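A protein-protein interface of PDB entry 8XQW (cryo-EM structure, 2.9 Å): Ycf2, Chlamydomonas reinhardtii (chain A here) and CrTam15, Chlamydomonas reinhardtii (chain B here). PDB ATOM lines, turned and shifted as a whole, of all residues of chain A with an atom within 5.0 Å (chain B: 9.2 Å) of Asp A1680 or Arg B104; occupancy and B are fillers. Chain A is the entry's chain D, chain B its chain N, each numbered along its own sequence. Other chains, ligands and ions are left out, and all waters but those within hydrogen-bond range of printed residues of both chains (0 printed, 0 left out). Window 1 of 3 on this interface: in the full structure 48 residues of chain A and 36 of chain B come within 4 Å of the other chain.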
ATOM      1  N   ILE A1672      28.758  22.286  19.362  1.00  0.00           N
ATOM      2  CA  ILE A1672      28.427  21.667  20.641  1.00  0.00           C
ATOM      3  C   ILE A1672      27.284  22.367  21.349  1.00  0.00           C
ATOM      4  O   ILE A1672      26.714  21.801  22.286  1.00  0.00           O
ATOM      5  CB  ILE A1672      29.618  21.641  21.612  1.00  0.00           C
ATOM      6  CG1 ILE A1672      30.048  23.065  21.939  1.00  0.00           C
ATOM      7  CG2 ILE A1672      30.759  20.836  21.035  1.00  0.00           C
ATOM      8  CD1 ILE A1672      31.091  23.135  23.008  1.00  0.00           C
ATOM      9  N   ILE A1675      23.941  20.875  19.356  1.00  0.00           N
ATOM     10  CA  ILE A1675      23.648  19.474  19.627  1.00  0.00           C
ATOM     11  C   ILE A1675      23.379  19.287  21.113  1.00  0.00           C
ATOM     12  O   ILE A1675      24.145  19.789  21.945  1.00  0.00           O
ATOM     13  CB  ILE A1675      24.799  18.580  19.156  1.00  0.00           C
ATOM     14  CG1 ILE A1675      24.942  18.671  17.643  1.00  0.00           C
ATOM     15  CG2 ILE A1675      24.551  17.165  19.543  1.00  0.00           C
ATOM     16  CD1 ILE A1675      25.838  17.621  17.060  1.00  0.00           C
ATOM     17  N   PRO A1676      22.318  18.581  21.493  1.00  0.00           N
ATOM     18  CA  PRO A1676      22.033  18.389  22.917  1.00  0.00           C
ATOM     19  C   PRO A1676      23.032  17.446  23.567  1.00  0.00           C
ATOM     20  O   PRO A1676      23.873  16.843  22.902  1.00  0.00           O
ATOM     21  CB  PRO A1676      20.626  17.782  22.917  1.00  0.00           C
ATOM     22  CG  PRO A1676      20.112  17.953  21.529  1.00  0.00           C
ATOM     23  CD  PRO A1676      21.289  17.968  20.644  1.00  0.00           C
ATOM     24  N   GLU A1677      22.939  17.333  24.890  1.00  0.00           N
ATOM     25  CA  GLU A1677      23.766  16.366  25.603  1.00  0.00           C
ATOM     26  C   GLU A1677      23.159  14.977  25.574  1.00  0.00           C
ATOM     27  O   GLU A1677      23.853  13.995  25.867  1.00  0.00           O
ATOM     28  CB  GLU A1677      23.961  16.798  27.050  1.00  0.00           C
ATOM     29  CG  GLU A1677      25.213  17.614  27.293  1.00  0.00           C
ATOM     30  CD  GLU A1677      25.793  17.384  28.673  1.00  0.00           C
ATOM     31  OE1 GLU A1677      25.211  16.589  29.439  1.00  0.00           O
ATOM     32  OE2 GLU A1677      26.831  17.996  28.994  1.00  0.00           O
ATOM     33  N   ASN A1678      21.876  14.881  25.233  1.00  0.00           N
ATOM     34  CA  ASN A1678      21.203  13.593  25.203  1.00  0.00           C
ATOM     35  C   ASN A1678      21.911  12.623  24.274  1.00  0.00           C
ATOM     36  O   ASN A1678      22.074  11.442  24.599  1.00  0.00           O
ATOM     37  CB  ASN A1678      19.756  13.793  24.771  1.00  0.00           C
ATOM     38  CG  ASN A1678      18.833  12.773  25.373  1.00  0.00           C
ATOM     39  OD1 ASN A1678      17.612  12.904  25.296  1.00  0.00           O
ATOM     40  ND2 ASN A1678      19.405  11.744  25.982  1.00  0.00           N
ATOM     41  N   VAL A1679      22.363  13.106  23.121  1.00  0.00           N
ATOM     42  CA  VAL A1679      22.984  12.208  22.161  1.00  0.00           C
ATOM     43  C   VAL A1679      24.362  11.775  22.640  1.00  0.00           C
ATOM     44  O   VAL A1679      24.779  10.635  22.413  1.00  0.00           O
ATOM     45  CB  VAL A1679      23.026  12.854  20.771  1.00  0.00           C
ATOM     46  CG1 VAL A1679      21.665  13.386  20.418  1.00  0.00           C
ATOM     47  CG2 VAL A1679      24.013  13.962  20.745  1.00  0.00           C
ATOM     48  N   ASP A1680      25.088  12.655  23.329  1.00  0.00           N
ATOM     49  CA  ASP A1680      26.375  12.245  23.873  1.00  0.00           C
ATOM     50  C   ASP A1680      26.191  11.167  24.923  1.00  0.00           C
ATOM     51  O   ASP A1680      26.941  10.184  24.961  1.00  0.00           O
ATOM     52  CB  ASP A1680      27.102  13.441  24.472  1.00  0.00           C
ATOM     53  CG  ASP A1680      27.036  14.656  23.589  1.00  0.00           C
ATOM     54  OD1 ASP A1680      26.650  14.511  22.415  1.00  0.00           O
ATOM     55  OD2 ASP A1680      27.369  15.759  24.064  1.00  0.00           O
ATOM     56  N   ILE A1681      25.177  11.319  25.770  1.00  0.00           N
ATOM     57  CA  ILE A1681      24.912  10.301  26.775  1.00  0.00           C
ATOM     58  C   ILE A1681      24.515   8.987  26.117  1.00  0.00           C
ATOM     59  O   ILE A1681      24.919   7.909  26.562  1.00  0.00           O
ATOM     60  CB  ILE A1681      23.845  10.803  27.757  1.00  0.00           C
ATOM     61  CG1 ILE A1681      24.462  11.859  28.664  1.00  0.00           C
ATOM     62  CG2 ILE A1681      23.284   9.668  28.556  1.00  0.00           C
ATOM     63  CD1 ILE A1681      23.455  12.669  29.401  1.00  0.00           C
ATOM     64  N   TYR A1682      23.747   9.051  25.030  1.00  0.00           N
ATOM     65  CA  TYR A1682      23.355   7.816  24.358  1.00  0.00           C
ATOM     66  C   TYR A1682      24.562   7.109  23.751  1.00  0.00           C
ATOM     67  O   TYR A1682      24.717   5.891  23.903  1.00  0.00           O
ATOM     68  CB  TYR A1682      22.306   8.110  23.292  1.00  0.00           C
ATOM     69  CG  TYR A1682      21.883   6.901  22.502  1.00  0.00           C
ATOM     70  CD1 TYR A1682      21.073   5.938  23.062  1.00  0.00           C
ATOM     71  CD2 TYR A1682      22.293   6.725  21.191  1.00  0.00           C
ATOM     72  CE1 TYR A1682      20.689   4.837  22.350  1.00  0.00           C
ATOM     73  CE2 TYR A1682      21.914   5.623  20.472  1.00  0.00           C
ATOM     74  CZ  TYR A1682      21.110   4.683  21.058  1.00  0.00           C
ATOM     75  OH  TYR A1682      20.720   3.574  20.357  1.00  0.00           O
ATOM     76  N   ILE A1683      25.427   7.855  23.068  1.00  0.00           N
ATOM     77  CA  ILE A1683      26.616   7.253  22.471  1.00  0.00           C
ATOM     78  C   ILE A1683      27.489   6.631  23.547  1.00  0.00           C
ATOM     79  O   ILE A1683      27.991   5.509  23.403  1.00  0.00           O
ATOM     80  CB  ILE A1683      27.400   8.297  21.660  1.00  0.00           C
ATOM     81  CG1 ILE A1683      26.517   8.947  20.606  1.00  0.00           C
ATOM     82  CG2 ILE A1683      28.569   7.649  20.987  1.00  0.00           C
ATOM     83  CD1 ILE A1683      26.245   8.078  19.428  1.00  0.00           C
ATOM     84  N   TRP A1684      27.690   7.356  24.644  1.00  0.00           N
ATOM     85  CA  TRP A1684      28.527   6.835  25.712  1.00  0.00           C
ATOM     86  C   TRP A1684      27.932   5.579  26.322  1.00  0.00           C
ATOM     87  O   TRP A1684      28.662   4.634  26.626  1.00  0.00           O
ATOM     88  CB  TRP A1684      28.733   7.898  26.781  1.00  0.00           C
ATOM     89  CG  TRP A1684      29.382   7.363  27.987  1.00  0.00           C
ATOM     90  CD1 TRP A1684      28.811   7.156  29.196  1.00  0.00           C
ATOM     91  CD2 TRP A1684      30.738   6.950  28.109  1.00  0.00           C
ATOM     92  NE1 TRP A1684      29.725   6.640  30.070  1.00  0.00           N
ATOM     93  CE2 TRP A1684      30.921   6.505  29.422  1.00  0.00           C
ATOM     94  CE3 TRP A1684      31.819   6.917  27.232  1.00  0.00           C
ATOM     95  CZ2 TRP A1684      32.133   6.028  29.880  1.00  0.00           C
ATOM     96  CZ3 TRP A1684      33.016   6.448  27.686  1.00  0.00           C
ATOM     97  CH2 TRP A1684      33.168   6.007  28.995  1.00  0.00           C
ATOM     98  N   ASN A1685      26.616   5.543  26.514  1.00  0.00           N
ATOM     99  CA  ASN A1685      25.989   4.356  27.078  1.00  0.00           C
ATOM    100  C   ASN A1685      26.191   3.152  26.180  1.00  0.00           C
ATOM    101  O   ASN A1685      26.544   2.065  26.648  1.00  0.00           O
ATOM    102  CB  ASN A1685      24.505   4.602  27.298  1.00  0.00           C
ATOM    103  CG  ASN A1685      24.228   5.291  28.593  1.00  0.00           C
ATOM    104  OD1 ASN A1685      25.029   5.236  29.521  1.00  0.00           O
ATOM    105  ND2 ASN A1685      23.088   5.956  28.673  1.00  0.00           N
ATOM    106  N   PHE A1755      36.596  11.781  21.204  1.00  0.00           N
ATOM    107  CA  PHE A1755      35.467  12.684  21.379  1.00  0.00           C
ATOM    108  C   PHE A1755      35.938  14.112  21.594  1.00  0.00           C
ATOM    109  O   PHE A1755      35.389  15.050  21.016  1.00  0.00           O
ATOM    110  CB  PHE A1755      34.614  12.220  22.550  1.00  0.00           C
ATOM    111  CG  PHE A1755      33.430  13.088  22.824  1.00  0.00           C
ATOM    112  CD1 PHE A1755      32.230  12.859  22.189  1.00  0.00           C
ATOM    113  CD2 PHE A1755      33.508  14.115  23.743  1.00  0.00           C
ATOM    114  CE1 PHE A1755      31.139  13.647  22.449  1.00  0.00           C
ATOM    115  CE2 PHE A1755      32.419  14.906  24.004  1.00  0.00           C
ATOM    116  CZ  PHE A1755      31.235  14.672  23.359  1.00  0.00           C
ATOM    117  N   TYR A1955      27.108  22.189  37.651  1.00  0.00           N
ATOM    118  CA  TYR A1955      26.777  22.058  36.244  1.00  0.00           C
ATOM    119  C   TYR A1955      25.344  22.508  36.017  1.00  0.00           C
ATOM    120  O   TYR A1955      24.529  22.503  36.937  1.00  0.00           O
ATOM    121  CB  TYR A1955      26.954  20.611  35.799  1.00  0.00           C
ATOM    122  CG  TYR A1955      27.207  20.428  34.338  1.00  0.00           C
ATOM    123  CD1 TYR A1955      28.383  20.861  33.763  1.00  0.00           C
ATOM    124  CD2 TYR A1955      26.281  19.796  33.533  1.00  0.00           C
ATOM    125  CE1 TYR A1955      28.619  20.690  32.421  1.00  0.00           C
ATOM    126  CE2 TYR A1955      26.511  19.616  32.191  1.00  0.00           C
ATOM    127  CZ  TYR A1955      27.680  20.066  31.640  1.00  0.00           C
ATOM    128  OH  TYR A1955      27.913  19.887  30.301  1.00  0.00           O
ATOM    129  N   PRO B 100      31.545   9.708  35.364  1.00  0.00           N
ATOM    130  CA  PRO B 100      30.149  10.123  35.262  1.00  0.00           C
ATOM    131  C   PRO B 100      29.556   9.671  33.939  1.00  0.00           C
ATOM    132  O   PRO B 100      30.245   9.163  33.055  1.00  0.00           O
ATOM    133  CB  PRO B 100      30.226  11.646  35.352  1.00  0.00           C
ATOM    134  CG  PRO B 100      31.544  11.933  35.900  1.00  0.00           C
ATOM    135  CD  PRO B 100      32.442  10.863  35.433  1.00  0.00           C
ATOM    136  N   THR B 101      28.252   9.869  33.798  1.00  0.00           N
ATOM    137  CA  THR B 101      27.572   9.388  32.606  1.00  0.00           C
ATOM    138  C   THR B 101      27.593  10.377  31.454  1.00  0.00           C
ATOM    139  O   THR B 101      27.304   9.980  30.326  1.00  0.00           O
ATOM    140  CB  THR B 101      26.128   9.035  32.932  1.00  0.00           C
ATOM    141  OG1 THR B 101      25.588  10.022  33.815  1.00  0.00           O
ATOM    142  CG2 THR B 101      26.064   7.688  33.605  1.00  0.00           C
ATOM    143  N   SER B 102      27.923  11.639  31.693  1.00  0.00           N
ATOM    144  CA  SER B 102      27.957  12.617  30.622  1.00  0.00           C
ATOM    145  C   SER B 102      29.394  13.003  30.334  1.00  0.00           C
ATOM    146  O   SER B 102      30.083  13.494  31.236  1.00  0.00           O
ATOM    147  CB  SER B 102      27.146  13.848  30.988  1.00  0.00           C
ATOM    148  OG  SER B 102      27.541  14.951  30.197  1.00  0.00           O
ATOM    149  N   PRO B 103      29.885  12.810  29.111  1.00  0.00           N
ATOM    150  CA  PRO B 103      31.304  13.069  28.840  1.00  0.00           C
ATOM    151  C   PRO B 103      31.696  14.528  28.920  1.00  0.00           C
ATOM    152  O   PRO B 103      32.892  14.823  29.014  1.00  0.00           O
ATOM    153  CB  PRO B 103      31.493  12.523  27.424  1.00  0.00           C
ATOM    154  CG  PRO B 103      30.359  11.589  27.222  1.00  0.00           C
ATOM    155  CD  PRO B 103      29.221  12.160  27.976  1.00  0.00           C
ATOM    156  N   ARG B 104      30.747  15.455  28.897  1.00  0.00           N
ATOM    157  CA  ARG B 104      31.121  16.858  28.981  1.00  0.00           C
ATOM    158  C   ARG B 104      31.543  17.259  30.385  1.00  0.00           C
ATOM    159  O   ARG B 104      32.440  18.090  30.536  1.00  0.00           O
ATOM    160  CB  ARG B 104      29.973  17.729  28.503  1.00  0.00           C
ATOM    161  CG  ARG B 104      29.517  17.391  27.111  1.00  0.00           C
ATOM    162  CD  ARG B 104      28.899  18.598  26.457  1.00  0.00           C
ATOM    163  NE  ARG B 104      28.098  18.243  25.293  1.00  0.00           N
ATOM    164  CZ  ARG B 104      27.426  19.124  24.566  1.00  0.00           C
ATOM    165  NH1 ARG B 104      27.463  20.407  24.891  1.00  0.00           N
ATOM    166  NH2 ARG B 104      26.715  18.726  23.523  1.00  0.00           N
ATOM    167  N   ILE B 105      30.912  16.693  31.415  1.00  0.00           N
ATOM    168  CA  ILE B 105      31.381  16.902  32.780  1.00  0.00           C
ATOM    169  C   ILE B 105      32.817  16.427  32.915  1.00  0.00           C
ATOM    170  O   ILE B 105      33.682  17.129  33.447  1.00  0.00           O
ATOM    171  CB  ILE B 105      30.465  16.177  33.780  1.00  0.00           C
ATOM    172  CG1 ILE B 105      29.168  16.936  33.982  1.00  0.00           C
ATOM    173  CG2 ILE B 105      31.140  16.060  35.104  1.00  0.00           C
ATOM    174  CD1 ILE B 105      28.075  16.498  33.087  1.00  0.00           C
ATOM    175  N   ARG B 106      33.091  15.231  32.406  1.00  0.00           N
ATOM    176  CA  ARG B 106      34.403  14.619  32.540  1.00  0.00           C
ATOM    177  C   ARG B 106      35.459  15.385  31.760  1.00  0.00           C
ATOM    178  O   ARG B 106      36.612  15.475  32.191  1.00  0.00           O
ATOM    179  CB  ARG B 106      34.312  13.177  32.065  1.00  0.00           C
ATOM    180  CG  ARG B 106      35.498  12.319  32.337  1.00  0.00           C
ATOM    181  CD  ARG B 106      35.229  10.957  31.763  1.00  0.00           C
ATOM    182  NE  ARG B 106      33.797  10.706  31.719  1.00  0.00           N
ATOM    183  CZ  ARG B 106      33.209   9.906  30.844  1.00  0.00           C
ATOM    184  NH1 ARG B 106      33.930   9.280  29.933  1.00  0.00           N
ATOM    185  NH2 ARG B 106      31.901   9.736  30.880  1.00  0.00           N
ATOM    186  N   LEU B 107      35.088  15.954  30.615  1.00  0.00           N
ATOM    187  CA  LEU B 107      36.044  16.592  29.720  1.00  0.00           C
ATOM    188  C   LEU B 107      36.094  18.108  29.841  1.00  0.00           C
ATOM    189  O   LEU B 107      36.915  18.732  29.168  1.00  0.00           O
ATOM    190  CB  LEU B 107      35.731  16.210  28.277  1.00  0.00           C
ATOM    191  CG  LEU B 107      36.093  14.771  27.954  1.00  0.00           C
ATOM    192  CD1 LEU B 107      35.529  14.379  26.622  1.00  0.00           C
ATOM    193  CD2 LEU B 107      37.590  14.620  27.959  1.00  0.00           C
ATOM    194  N   GLN B 108      35.245  18.715  30.670  1.00  0.00           N
ATOM    195  CA  GLN B 108      35.258  20.159  30.907  1.00  0.00           C
ATOM    196  C   GLN B 108      35.063  20.942  29.607  1.00  0.00           C
ATOM    197  O   GLN B 108      35.935  21.686  29.159  1.00  0.00           O
ATOM    198  CB  GLN B 108      36.545  20.586  31.615  1.00  0.00           C
ATOM    199  CG  GLN B 108      36.586  20.259  33.091  1.00  0.00           C
ATOM    200  CD  GLN B 108      37.815  19.457  33.476  1.00  0.00           C
ATOM    201  OE1 GLN B 108      38.941  19.933  33.363  1.00  0.00           O
ATOM    202  NE2 GLN B 108      37.599  18.236  33.939  1.00  0.00           N
ATOM    203  N   ILE B 109      33.889  20.770  29.010  1.00  0.00           N
ATOM    204  CA  ILE B 109      33.547  21.394  27.736  1.00  0.00           C
ATOM    205  C   ILE B 109      32.371  22.332  27.954  1.00  0.00           C
ATOM    206  O   ILE B 109      31.368  21.945  28.566  1.00  0.00           O
ATOM    207  CB  ILE B 109      33.217  20.337  26.674  1.00  0.00           C
ATOM    208  CG1 ILE B 109      34.499  19.720  26.128  1.00  0.00           C
ATOM    209  CG2 ILE B 109      32.411  20.942  25.565  1.00  0.00           C
ATOM    210  CD1 ILE B 109      34.271  18.787  24.980  1.00  0.00           C
ATOM    211  N   ARG B 110      32.490  23.560  27.454  1.00  0.00           N
ATOM    212  CA  ARG B 110      31.425  24.544  27.577  1.00  0.00           C
ATOM    213  C   ARG B 110      31.598  25.586  26.482  1.00  0.00           C
ATOM    214  O   ARG B 110      32.706  25.744  25.959  1.00  0.00           O
ATOM    215  CB  ARG B 110      31.444  25.204  28.959  1.00  0.00           C
ATOM    216  CG  ARG B 110      32.785  25.753  29.376  1.00  0.00           C
ATOM    217  CD  ARG B 110      32.709  26.362  30.769  1.00  0.00           C
ATOM    218  NE  ARG B 110      31.887  27.570  30.809  1.00  0.00           N
ATOM    219  CZ  ARG B 110      30.599  27.601  31.141  1.00  0.00           C
ATOM    220  NH1 ARG B 110      29.962  26.485  31.466  1.00  0.00           N
ATOM    221  NH2 ARG B 110      29.944  28.751  31.148  1.00  0.00           N
ATOM    222  N   PRO B 111      30.536  26.302  26.111  1.00  0.00           N
ATOM    223  CA  PRO B 111      30.635  27.242  24.991  1.00  0.00           C
ATOM    224  C   PRO B 111      31.445  28.480  25.348  1.00  0.00           C
ATOM    225  O   PRO B 111      31.820  28.708  26.500  1.00  0.00           O
ATOM    226  CB  PRO B 111      29.174  27.605  24.700  1.00  0.00           C
ATOM    227  CG  PRO B 111      28.360  26.580  25.418  1.00  0.00           C
ATOM    228  CD  PRO B 111      29.157  26.210  26.611  1.00  0.00           C
ATOM    229  N   TYR B 124      18.048  23.742  18.024  1.00  0.00           N
ATOM    230  CA  TYR B 124      18.375  22.923  19.185  1.00  0.00           C
ATOM    231  C   TYR B 124      17.185  22.067  19.578  1.00  0.00           C
ATOM    232  O   TYR B 124      17.262  20.832  19.589  1.00  0.00           O
ATOM    233  CB  TYR B 124      18.796  23.833  20.342  1.00  0.00           C
ATOM    234  CG  TYR B 124      19.201  23.138  21.621  1.00  0.00           C
ATOM    235  CD1 TYR B 124      18.259  22.552  22.449  1.00  0.00           C
ATOM    236  CD2 TYR B 124      20.522  23.114  22.022  1.00  0.00           C
ATOM    237  CE1 TYR B 124      18.625  21.936  23.619  1.00  0.00           C
ATOM    238  CE2 TYR B 124      20.898  22.499  23.189  1.00  0.00           C
ATOM    239  CZ  TYR B 124      19.944  21.912  23.983  1.00  0.00           C
ATOM    240  OH  TYR B 124      20.317  21.297  25.151  1.00  0.00           O
ATOM    241  N   SER B 131      15.637  13.257  19.275  1.00  0.00           N
ATOM    242  CA  SER B 131      16.474  12.319  20.064  1.00  0.00           C
ATOM    243  C   SER B 131      15.607  11.596  21.093  1.00  0.00           C
ATOM    244  O   SER B 131      15.834  10.398  21.315  1.00  0.00           O
ATOM    245  CB  SER B 131      17.582  13.058  20.754  1.00  0.00           C
ATOM    246  OG  SER B 131      17.237  13.361  22.099  1.00  0.00           O
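NH2 of Arg B104 is in hydrogen-bond range of O of Pro A1676.
The guanidinium group (NH2) of Arg B104 sits at hydrogen-bond distance from the backbone carbonyl oxygen (O) of Ile A1675, at 3.2 Å.
The side-chain carboxylate (OD2) of Asp A1680 lies within salt-bridge range of the guanidinium group (NE) of Arg B104, at 2.9 Å.
The guanidinium group (NE) of Arg B104 lies within salt-bridge range of the side-chain carboxylate (OE2) of Glu A1677, at 3.9 Å.
OG of Ser B102 sits at hydrogen-bond distance from OE1 of Glu A1677 (2.9 Å).
The backbone carbonyl oxygen (O) of Ile A1672 lies within hydrogen-bond range of the guanidinium group (NH1) of Arg B104.
The side-chain hydroxyl of Ser B131 is in hydrogen-bond range of the side-chain amide oxygen of Asn A1678.
O of Arg B104 lies within hydrogen-bond range of N of Ile B109, at 3.4 Å.
The side-chain carboxylate of Glu A1677 lies within hydrogen-bond range of the side-chain hydroxyl of Tyr A1955, 2.5 Å away.
The backbone carbonyl oxygen (O) of Pro B100 is in hydrogen-bond range of the guanidinium group (NH2) of Arg B106, 2.8 Å away.
O of Arg B106 lies within hydrogen-bond range of NE2 of Gln B108, 3.4 Å away.
The backbone carbonyl oxygen of Ile A1681 sits close to the side-chain amide nitrogen of Asn A1685 (3.4 Å).
The side-chain hydroxyl of Ser B102 sits close to the backbone NH of Arg B104, 3.5 Å away.
Ile B109 touches Ile A1672 (CG2 to CD1, 3.6 Å).
Ile A1681 touches Thr B101 (CG1 to O, 3.8 Å).
Pro B100 touches Trp A1684 (O to NE1, 3.9 Å).
Thr B101 touches Trp A1684.
Trp A1684 touches Arg B106.
CD2 of Phe A1755 touches CD1 of Leu B107, 3.5 Å away.
Arg B104 touches Tyr A1955 (CB to OH, 3.5 Å).
CE2 of Tyr A1955 touches CD1 of Ile B105, at 3.6 Å.
Of the printed residues of chain B, Ile A1672 touches Arg B104 (3.0 Å) and Ile B109 (3.6 Å).
Of the printed residues of chain B, Glu A1677 touches Ser B102 (2.9 Å) and Arg B104 (3.2 Å).
Val A1679 touches none of the printed residues of chain B.
Asp A1680 touches just one residue of chain B: Arg B104.
Printed residues of chain B within 4 Å of Ile A1681: Thr B101.
Printed residues of chain B within 4 Å of Trp A1684: Pro B100, Thr B101 and Arg B106.
Printed residues of chain A within 4 Å of Pro B100: Trp A1684.
Arg B104 touches just these residues of chain A: Ile A1672, Ile A1675, Pro A1676, Glu A1677, Asp A1680 and Tyr A1955.
Gln B108 touches none of the printed residues of chain A.
Pro B111 touches none of the printed residues of chain A.
Of the printed residues of chain A, Ser B131 touches Asn A1678.
The nearest residue of chain A that does not touch Arg B104 is Phe A1755 (4.9 Å).
The nearest printed residue of chain A that does not touch Pro B100 is Asn A1685 (7.4 Å).
Printed residues of chain B that touch a printed residue of chain A: Pro B100, Thr B101, Ser B102, Arg B104, Ile B105, Arg B106, Leu B107, Ile B109 and Ser B131.
Hydrophobic or aromatic side chains of chain A that line the printed part of chain B: Ile A1672, Ile A1681, Trp A1684, Phe A1755 and Tyr A1955.
Among the printed residues, Asp or Glu carboxylates within 4 Å of a Lys or Arg side-chain nitrogen of the other chain: Glu A1677 with Arg B104 and Asp A1680 with Arg B104.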
